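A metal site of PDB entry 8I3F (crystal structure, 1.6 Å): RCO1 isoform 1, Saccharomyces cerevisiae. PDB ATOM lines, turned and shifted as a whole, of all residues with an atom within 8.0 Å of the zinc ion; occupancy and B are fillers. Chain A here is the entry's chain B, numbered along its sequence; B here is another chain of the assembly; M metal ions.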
ATOM      1  N   PHE A   5       0.865 -26.251  28.667  1.00  0.00           N
ATOM      2  CA  PHE A   5       1.714 -25.578  27.712  1.00  0.00           C
ATOM      3  C   PHE A   5       1.064 -24.239  27.416  1.00  0.00           C
ATOM      4  O   PHE A   5      -0.135 -24.053  27.636  1.00  0.00           O
ATOM      5  CB  PHE A   5       1.862 -26.413  26.427  1.00  0.00           C
ATOM      6  CG  PHE A   5       0.523 -26.738  25.782  1.00  0.00           C
ATOM      7  CD1 PHE A   5      -0.193 -27.856  26.163  1.00  0.00           C
ATOM      8  CD2 PHE A   5      -0.023 -25.897  24.802  1.00  0.00           C
ATOM      9  CE1 PHE A   5      -1.423 -28.160  25.588  1.00  0.00           C
ATOM     10  CE2 PHE A   5      -1.246 -26.189  24.224  1.00  0.00           C
ATOM     11  CZ  PHE A   5      -1.953 -27.333  24.621  1.00  0.00           C
ATOM     12  N   CYS A   6       1.881 -23.309  26.936  1.00  0.00           N
ATOM     13  CA  CYS A   6       1.367 -22.012  26.476  1.00  0.00           C
ATOM     14  C   CYS A   6       0.617 -22.167  25.163  1.00  0.00           C
ATOM     15  O   CYS A   6       1.147 -22.714  24.189  1.00  0.00           O
ATOM     16  CB  CYS A   6       2.520 -21.038  26.325  1.00  0.00           C
ATOM     17  SG  CYS A   6       2.003 -19.358  25.803  1.00  0.00           S
ATOM     18  N   SER A   7      -0.613 -21.649  25.103  1.00  0.00           N
ATOM     19  CA  SER A   7      -1.369 -21.747  23.855  1.00  0.00           C
ATOM     20  C   SER A   7      -0.738 -20.912  22.764  1.00  0.00           C
ATOM     21  O   SER A   7      -0.863 -21.245  21.585  1.00  0.00           O
ATOM     22  CB  SER A   7      -2.826 -21.296  24.063  1.00  0.00           C
ATOM     23  OG  SER A   7      -3.596 -22.394  24.523  1.00  0.00           O
ATOM     24  N   ALA A   8      -0.044 -19.839  23.139  1.00  0.00           N
ATOM     25  CA  ALA A   8       0.495 -18.968  22.106  1.00  0.00           C
ATOM     26  C   ALA A   8       1.761 -19.540  21.467  1.00  0.00           C
ATOM     27  O   ALA A   8       1.927 -19.447  20.238  1.00  0.00           O
ATOM     28  CB  ALA A   8       0.750 -17.574  22.677  1.00  0.00           C
ATOM     29  N   CYS A   9       2.673 -20.133  22.257  1.00  0.00           N
ATOM     30  CA  CYS A   9       3.963 -20.568  21.696  1.00  0.00           C
ATOM     31  C   CYS A   9       4.249 -22.059  21.879  1.00  0.00           C
ATOM     32  O   CYS A   9       5.315 -22.530  21.452  1.00  0.00           O
ATOM     33  CB  CYS A   9       5.103 -19.733  22.310  1.00  0.00           C
ATOM     34  SG  CYS A   9       5.389 -20.197  24.090  1.00  0.00           S
ATOM     35  N   ASN A  10       3.356 -22.789  22.548  1.00  0.00           N
ATOM     36  CA  ASN A  10       3.377 -24.247  22.716  1.00  0.00           C
ATOM     37  C   ASN A  10       4.491 -24.716  23.641  1.00  0.00           C
ATOM     38  O   ASN A  10       4.745 -25.920  23.693  1.00  0.00           O
ATOM     39  CB  ASN A  10       3.459 -24.964  21.369  1.00  0.00           C
ATOM     40  CG  ASN A  10       2.179 -24.811  20.590  1.00  0.00           C
ATOM     41  OD1 ASN A  10       1.079 -25.087  21.111  1.00  0.00           O
ATOM     42  ND2 ASN A  10       2.293 -24.338  19.354  1.00  0.00           N
ATOM     43  N   GLN A  11       5.133 -23.813  24.369  1.00  0.00           N
ATOM     44  CA  GLN A  11       6.234 -24.189  25.244  1.00  0.00           C
ATOM     45  C   GLN A  11       5.793 -24.265  26.714  1.00  0.00           C
ATOM     46  O   GLN A  11       4.724 -23.792  27.117  1.00  0.00           O
ATOM     47  CB  GLN A  11       7.407 -23.221  25.085  1.00  0.00           C
ATOM     48  CG  GLN A  11       7.951 -23.119  23.637  1.00  0.00           C
ATOM     49  CD  GLN A  11       8.024 -24.459  22.908  1.00  0.00           C
ATOM     50  OE1 GLN A  11       8.647 -25.399  23.388  1.00  0.00           O
ATOM     51  NE2 GLN A  11       7.378 -24.544  21.738  1.00  0.00           N
ATOM     52  N   SER A  12       6.662 -24.892  27.505  1.00  0.00           N
ATOM     53  CA  SER A  12       6.480 -25.099  28.932  1.00  0.00           C
ATOM     54  C   SER A  12       6.815 -23.840  29.723  1.00  0.00           C
ATOM     55  O   SER A  12       7.281 -22.852  29.179  1.00  0.00           O
ATOM     56  CB  SER A  12       7.353 -26.262  29.408  1.00  0.00           C
ATOM     57  OG  SER A  12       8.715 -25.882  29.307  1.00  0.00           O
ATOM     58  N   SER A  14       5.846 -21.020  33.176  1.00  0.00           N
ATOM     59  CA  SER A  14       4.890 -20.418  34.108  1.00  0.00           C
ATOM     60  C   SER A  14       3.793 -19.720  33.330  1.00  0.00           C
ATOM     61  O   SER A  14       4.076 -18.958  32.409  1.00  0.00           O
ATOM     62  CB  SER A  14       5.566 -19.416  35.054  1.00  0.00           C
ATOM     63  OG  SER A  14       6.717 -19.973  35.654  1.00  0.00           O
ATOM     64  N   PHE A  15       2.539 -20.015  33.708  1.00  0.00           N
ATOM     65  CA  PHE A  15       1.384 -19.542  32.967  1.00  0.00           C
ATOM     66  C   PHE A  15       0.379 -18.825  33.860  1.00  0.00           C
ATOM     67  O   PHE A  15       0.252 -19.084  35.058  1.00  0.00           O
ATOM     68  CB  PHE A  15       0.612 -20.673  32.269  1.00  0.00           C
ATOM     69  CG  PHE A  15       1.493 -21.699  31.616  1.00  0.00           C
ATOM     70  CD1 PHE A  15       2.329 -21.345  30.554  1.00  0.00           C
ATOM     71  CD2 PHE A  15       1.471 -23.012  32.066  1.00  0.00           C
ATOM     72  CE1 PHE A  15       3.129 -22.304  29.943  1.00  0.00           C
ATOM     73  CE2 PHE A  15       2.251 -23.983  31.461  1.00  0.00           C
ATOM     74  CZ  PHE A  15       3.088 -23.636  30.406  1.00  0.00           C
ATOM     75  N   SER A  24      -3.807 -21.891  28.841  1.00  0.00           N
ATOM     76  CA  SER A  24      -2.833 -21.238  29.706  1.00  0.00           C
ATOM     77  C   SER A  24      -1.860 -20.492  28.825  1.00  0.00           C
ATOM     78  O   SER A  24      -1.623 -20.886  27.691  1.00  0.00           O
ATOM     79  CB  SER A  24      -2.055 -22.200  30.548  1.00  0.00           C
ATOM     80  OG  SER A  24      -2.921 -23.039  31.263  1.00  0.00           O
ATOM     81  N   PHE A  25      -1.285 -19.431  29.381  1.00  0.00           N
ATOM     82  CA  PHE A  25      -0.416 -18.542  28.587  1.00  0.00           C
ATOM     83  C   PHE A  25       0.761 -18.055  29.411  1.00  0.00           C
ATOM     84  O   PHE A  25       0.570 -17.695  30.577  1.00  0.00           O
ATOM     85  CB  PHE A  25      -1.189 -17.317  28.112  1.00  0.00           C
ATOM     86  CG  PHE A  25      -2.210 -17.591  27.066  1.00  0.00           C
ATOM     87  CD1 PHE A  25      -3.512 -17.939  27.404  1.00  0.00           C
ATOM     88  CD2 PHE A  25      -1.875 -17.428  25.715  1.00  0.00           C
ATOM     89  CE1 PHE A  25      -4.450 -18.188  26.395  1.00  0.00           C
ATOM     90  CE2 PHE A  25      -2.782 -17.673  24.719  1.00  0.00           C
ATOM     91  CZ  PHE A  25      -4.073 -18.025  25.038  1.00  0.00           C
ATOM     92  N   HIS A  26       1.964 -17.997  28.803  1.00  0.00           N
ATOM     93  CA  HIS A  26       3.045 -17.253  29.453  1.00  0.00           C
ATOM     94  C   HIS A  26       2.614 -15.810  29.635  1.00  0.00           C
ATOM     95  O   HIS A  26       1.957 -15.248  28.772  1.00  0.00           O
ATOM     96  CB  HIS A  26       4.322 -17.266  28.583  1.00  0.00           C
ATOM     97  CG  HIS A  26       4.977 -18.598  28.428  1.00  0.00           C
ATOM     98  ND1 HIS A  26       5.132 -19.207  27.208  1.00  0.00           N
ATOM     99  CD2 HIS A  26       5.492 -19.460  29.340  1.00  0.00           C
ATOM    100  CE1 HIS A  26       5.768 -20.361  27.348  1.00  0.00           C
ATOM    101  NE2 HIS A  26       5.990 -20.547  28.644  1.00  0.00           N
ATOM    102  N   PHE A  27       3.037 -15.184  30.753  1.00  0.00           N
ATOM    103  CA  PHE A  27       2.692 -13.772  30.991  1.00  0.00           C
ATOM    104  C   PHE A  27       3.091 -12.885  29.816  1.00  0.00           C
ATOM    105  O   PHE A  27       2.320 -12.009  29.407  1.00  0.00           O
ATOM    106  CB  PHE A  27       3.374 -13.259  32.281  1.00  0.00           C
ATOM    107  CG  PHE A  27       3.072 -14.098  33.486  1.00  0.00           C
ATOM    108  CD1 PHE A  27       1.784 -14.174  33.942  1.00  0.00           C
ATOM    109  CD2 PHE A  27       4.067 -14.828  34.142  1.00  0.00           C
ATOM    110  CE1 PHE A  27       1.463 -14.939  35.053  1.00  0.00           C
ATOM    111  CE2 PHE A  27       3.746 -15.599  35.261  1.00  0.00           C
ATOM    112  CZ  PHE A  27       2.434 -15.643  35.694  1.00  0.00           C
ATOM    113  N   LEU A  28       4.262 -13.130  29.225  1.00  0.00           N
ATOM    114  CA  LEU A  28       4.730 -12.277  28.145  1.00  0.00           C
ATOM    115  C   LEU A  28       4.077 -12.611  26.808  1.00  0.00           C
ATOM    116  O   LEU A  28       4.145 -11.782  25.882  1.00  0.00           O
ATOM    117  CB  LEU A  28       6.254 -12.389  28.015  1.00  0.00           C
ATOM    118  CG  LEU A  28       7.052 -11.539  29.011  1.00  0.00           C
ATOM    119  CD1 LEU A  28       8.558 -11.978  28.956  1.00  0.00           C
ATOM    120  CD2 LEU A  28       6.941 -10.094  28.642  1.00  0.00           C
ATOM    121  N   CYS A  29       3.444 -13.775  26.680  1.00  0.00           N
ATOM    122  CA  CYS A  29       2.788 -14.140  25.423  1.00  0.00           C
ATOM    123  C   CYS A  29       1.399 -13.549  25.289  1.00  0.00           C
ATOM    124  O   CYS A  29       0.814 -13.625  24.198  1.00  0.00           O
ATOM    125  CB  CYS A  29       2.706 -15.676  25.294  1.00  0.00           C
ATOM    126  SG  CYS A  29       4.351 -16.432  24.871  1.00  0.00           S
ATOM    127  N   LEU A  30       0.886 -12.929  26.338  1.00  0.00           N
ATOM    128  CA  LEU A  30      -0.417 -12.316  26.319  1.00  0.00           C
ATOM    129  C   LEU A  30      -0.338 -10.975  25.604  1.00  0.00           C
ATOM    130  O   LEU A  30       0.742 -10.404  25.427  1.00  0.00           O
ATOM    131  CB  LEU A  30      -0.951 -12.130  27.739  1.00  0.00           C
ATOM    132  CG  LEU A  30      -1.288 -13.491  28.337  1.00  0.00           C
ATOM    133  CD1 LEU A  30      -1.548 -13.322  29.839  1.00  0.00           C
ATOM    134  CD2 LEU A  30      -2.486 -14.076  27.617  1.00  0.00           C
ATOM    135  N   PRO A  91      -3.837 -14.449  21.245  1.00  0.00           N
ATOM    136  CA  PRO A  91      -2.509 -14.175  20.664  1.00  0.00           C
ATOM    137  C   PRO A  91      -1.765 -15.464  20.428  1.00  0.00           C
ATOM    138  O   PRO A  91      -1.989 -16.483  21.085  1.00  0.00           O
ATOM    139  CB  PRO A  91      -1.823 -13.308  21.731  1.00  0.00           C
ATOM    140  CG  PRO A  91      -2.562 -13.562  22.990  1.00  0.00           C
ATOM    141  CD  PRO A  91      -3.991 -13.870  22.586  1.00  0.00           C
ATOM    142  N   LYS A  92      -0.860 -15.416  19.448  1.00  0.00           N
ATOM    143  CA  LYS A  92      -0.025 -16.565  19.148  1.00  0.00           C
ATOM    144  C   LYS A  92       1.352 -16.082  18.733  1.00  0.00           C
ATOM    145  O   LYS A  92       1.539 -14.916  18.344  1.00  0.00           O
ATOM    146  CB  LYS A  92      -0.632 -17.416  18.032  1.00  0.00           C
ATOM    147  CG  LYS A  92      -0.614 -16.796  16.671  1.00  0.00           C
ATOM    148  CD  LYS A  92      -1.437 -17.649  15.703  1.00  0.00           C
ATOM    149  CE  LYS A  92      -1.669 -16.899  14.397  1.00  0.00           C
ATOM    150  NZ  LYS A  92      -2.812 -17.436  13.605  1.00  0.00           N
ATOM    151  N   GLN A  93       2.308 -16.977  18.817  1.00  0.00           N
ATOM    152  CA  GLN A  93       3.646 -16.683  18.320  1.00  0.00           C
ATOM    153  C   GLN A  93       3.659 -16.649  16.790  1.00  0.00           C
ATOM    154  O   GLN A  93       3.040 -17.477  16.124  1.00  0.00           O
ATOM    155  CB  GLN A  93       4.616 -17.763  18.830  1.00  0.00           C
ATOM    156  CG  GLN A  93       6.084 -17.412  18.446  1.00  0.00           C
ATOM    157  CD  GLN A  93       7.128 -18.391  18.928  1.00  0.00           C
ATOM    158  OE1 GLN A  93       8.255 -17.986  19.216  1.00  0.00           O
ATOM    159  NE2 GLN A  93       6.770 -19.706  19.045  1.00  0.00           N
ATOM    160  N   ARG B  83       8.629 -15.328  20.127  1.00  0.00           N
ATOM    161  CA  ARG B  83       8.598 -15.243  21.577  1.00  0.00           C
ATOM    162  C   ARG B  83       9.679 -14.296  22.124  1.00  0.00           C
ATOM    163  O   ARG B  83       9.414 -13.515  23.054  1.00  0.00           O
ATOM    164  CB  ARG B  83       8.746 -16.655  22.172  1.00  0.00           C
ATOM    165  CG  ARG B  83       8.544 -16.644  23.674  1.00  0.00           C
ATOM    166  CD  ARG B  83       8.468 -18.056  24.245  1.00  0.00           C
ATOM    167  NE  ARG B  83       8.372 -17.912  25.689  1.00  0.00           N
ATOM    168  CZ  ARG B  83       8.756 -18.828  26.571  1.00  0.00           C
ATOM    169  NH1 ARG B  83       9.286 -19.965  26.123  1.00  0.00           N
ATOM    170  NH2 ARG B  83       8.627 -18.617  27.878  1.00  0.00           N
ATOM    171  N   ARG B  86       8.824 -10.606  22.612  1.00  0.00           N
ATOM    172  CA  ARG B  86       7.735 -10.133  23.460  1.00  0.00           C
ATOM    173  C   ARG B  86       8.183  -9.301  24.663  1.00  0.00           C
ATOM    174  O   ARG B  86       7.429  -8.485  25.140  1.00  0.00           O
ATOM    175  CB  ARG B  86       6.779 -11.274  23.800  1.00  0.00           C
ATOM    176  CG  ARG B  86       6.213 -11.864  22.519  1.00  0.00           C
ATOM    177  CD  ARG B  86       4.870 -12.532  22.699  1.00  0.00           C
ATOM    178  NE  ARG B  86       3.853 -11.626  23.183  1.00  0.00           N
ATOM    179  CZ  ARG B  86       3.007 -10.966  22.405  1.00  0.00           C
ATOM    180  NH1 ARG B  86       3.063 -11.089  21.092  1.00  0.00           N
ATOM    181  NH2 ARG B  86       2.105 -10.173  22.949  1.00  0.00           N
ATOM    182  N   ALA B 181      13.072 -13.365  28.633  1.00  0.00           N
ATOM    183  CA  ALA B 181      12.092 -13.522  27.578  1.00  0.00           C
ATOM    184  C   ALA B 181      11.715 -14.984  27.326  1.00  0.00           C
ATOM    185  O   ALA B 181      10.580 -15.250  26.934  1.00  0.00           O
ATOM    186  CB  ALA B 181      12.639 -12.915  26.283  1.00  0.00           C
HETATM  187 ZN    ZN M   1       4.218 -18.649  25.367  1.00  0.00          ZN
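A ring nitrogen (NE2) of His 26 sits at hydrogen-bond distance from the guanidinium group (NH2) of Arg 83 of chain B (3.4 Å).
The backbone carbonyl oxygen of Ser 12 sits at hydrogen-bond distance from a ring nitrogen (NE2) of His 26 (2.7 Å).
The backbone carbonyl oxygen of Cys 9 lies within hydrogen-bond range of the side-chain amide nitrogen of Gln 11, 2.9 Å away.
The side-chain sulfur (SG) of Cys 6 lies close to the backbone NH (N) of Ala 8, 3.4 Å away.
The backbone NH (N) of Cys 6 sits at hydrogen-bond distance from the backbone carbonyl oxygen (O) of Gln 11 (2.9 Å).
ND1 of His 26 is bound to the zinc ion (2.1 Å).
SG of Cys 29 binds the zinc ion (2.3 Å).
The side-chain sulfur (SG) of Cys 9 is bound to the zinc ion, 2.3 Å away.
The zinc ion is bound by SG of Cys 6, 2.4 Å away.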
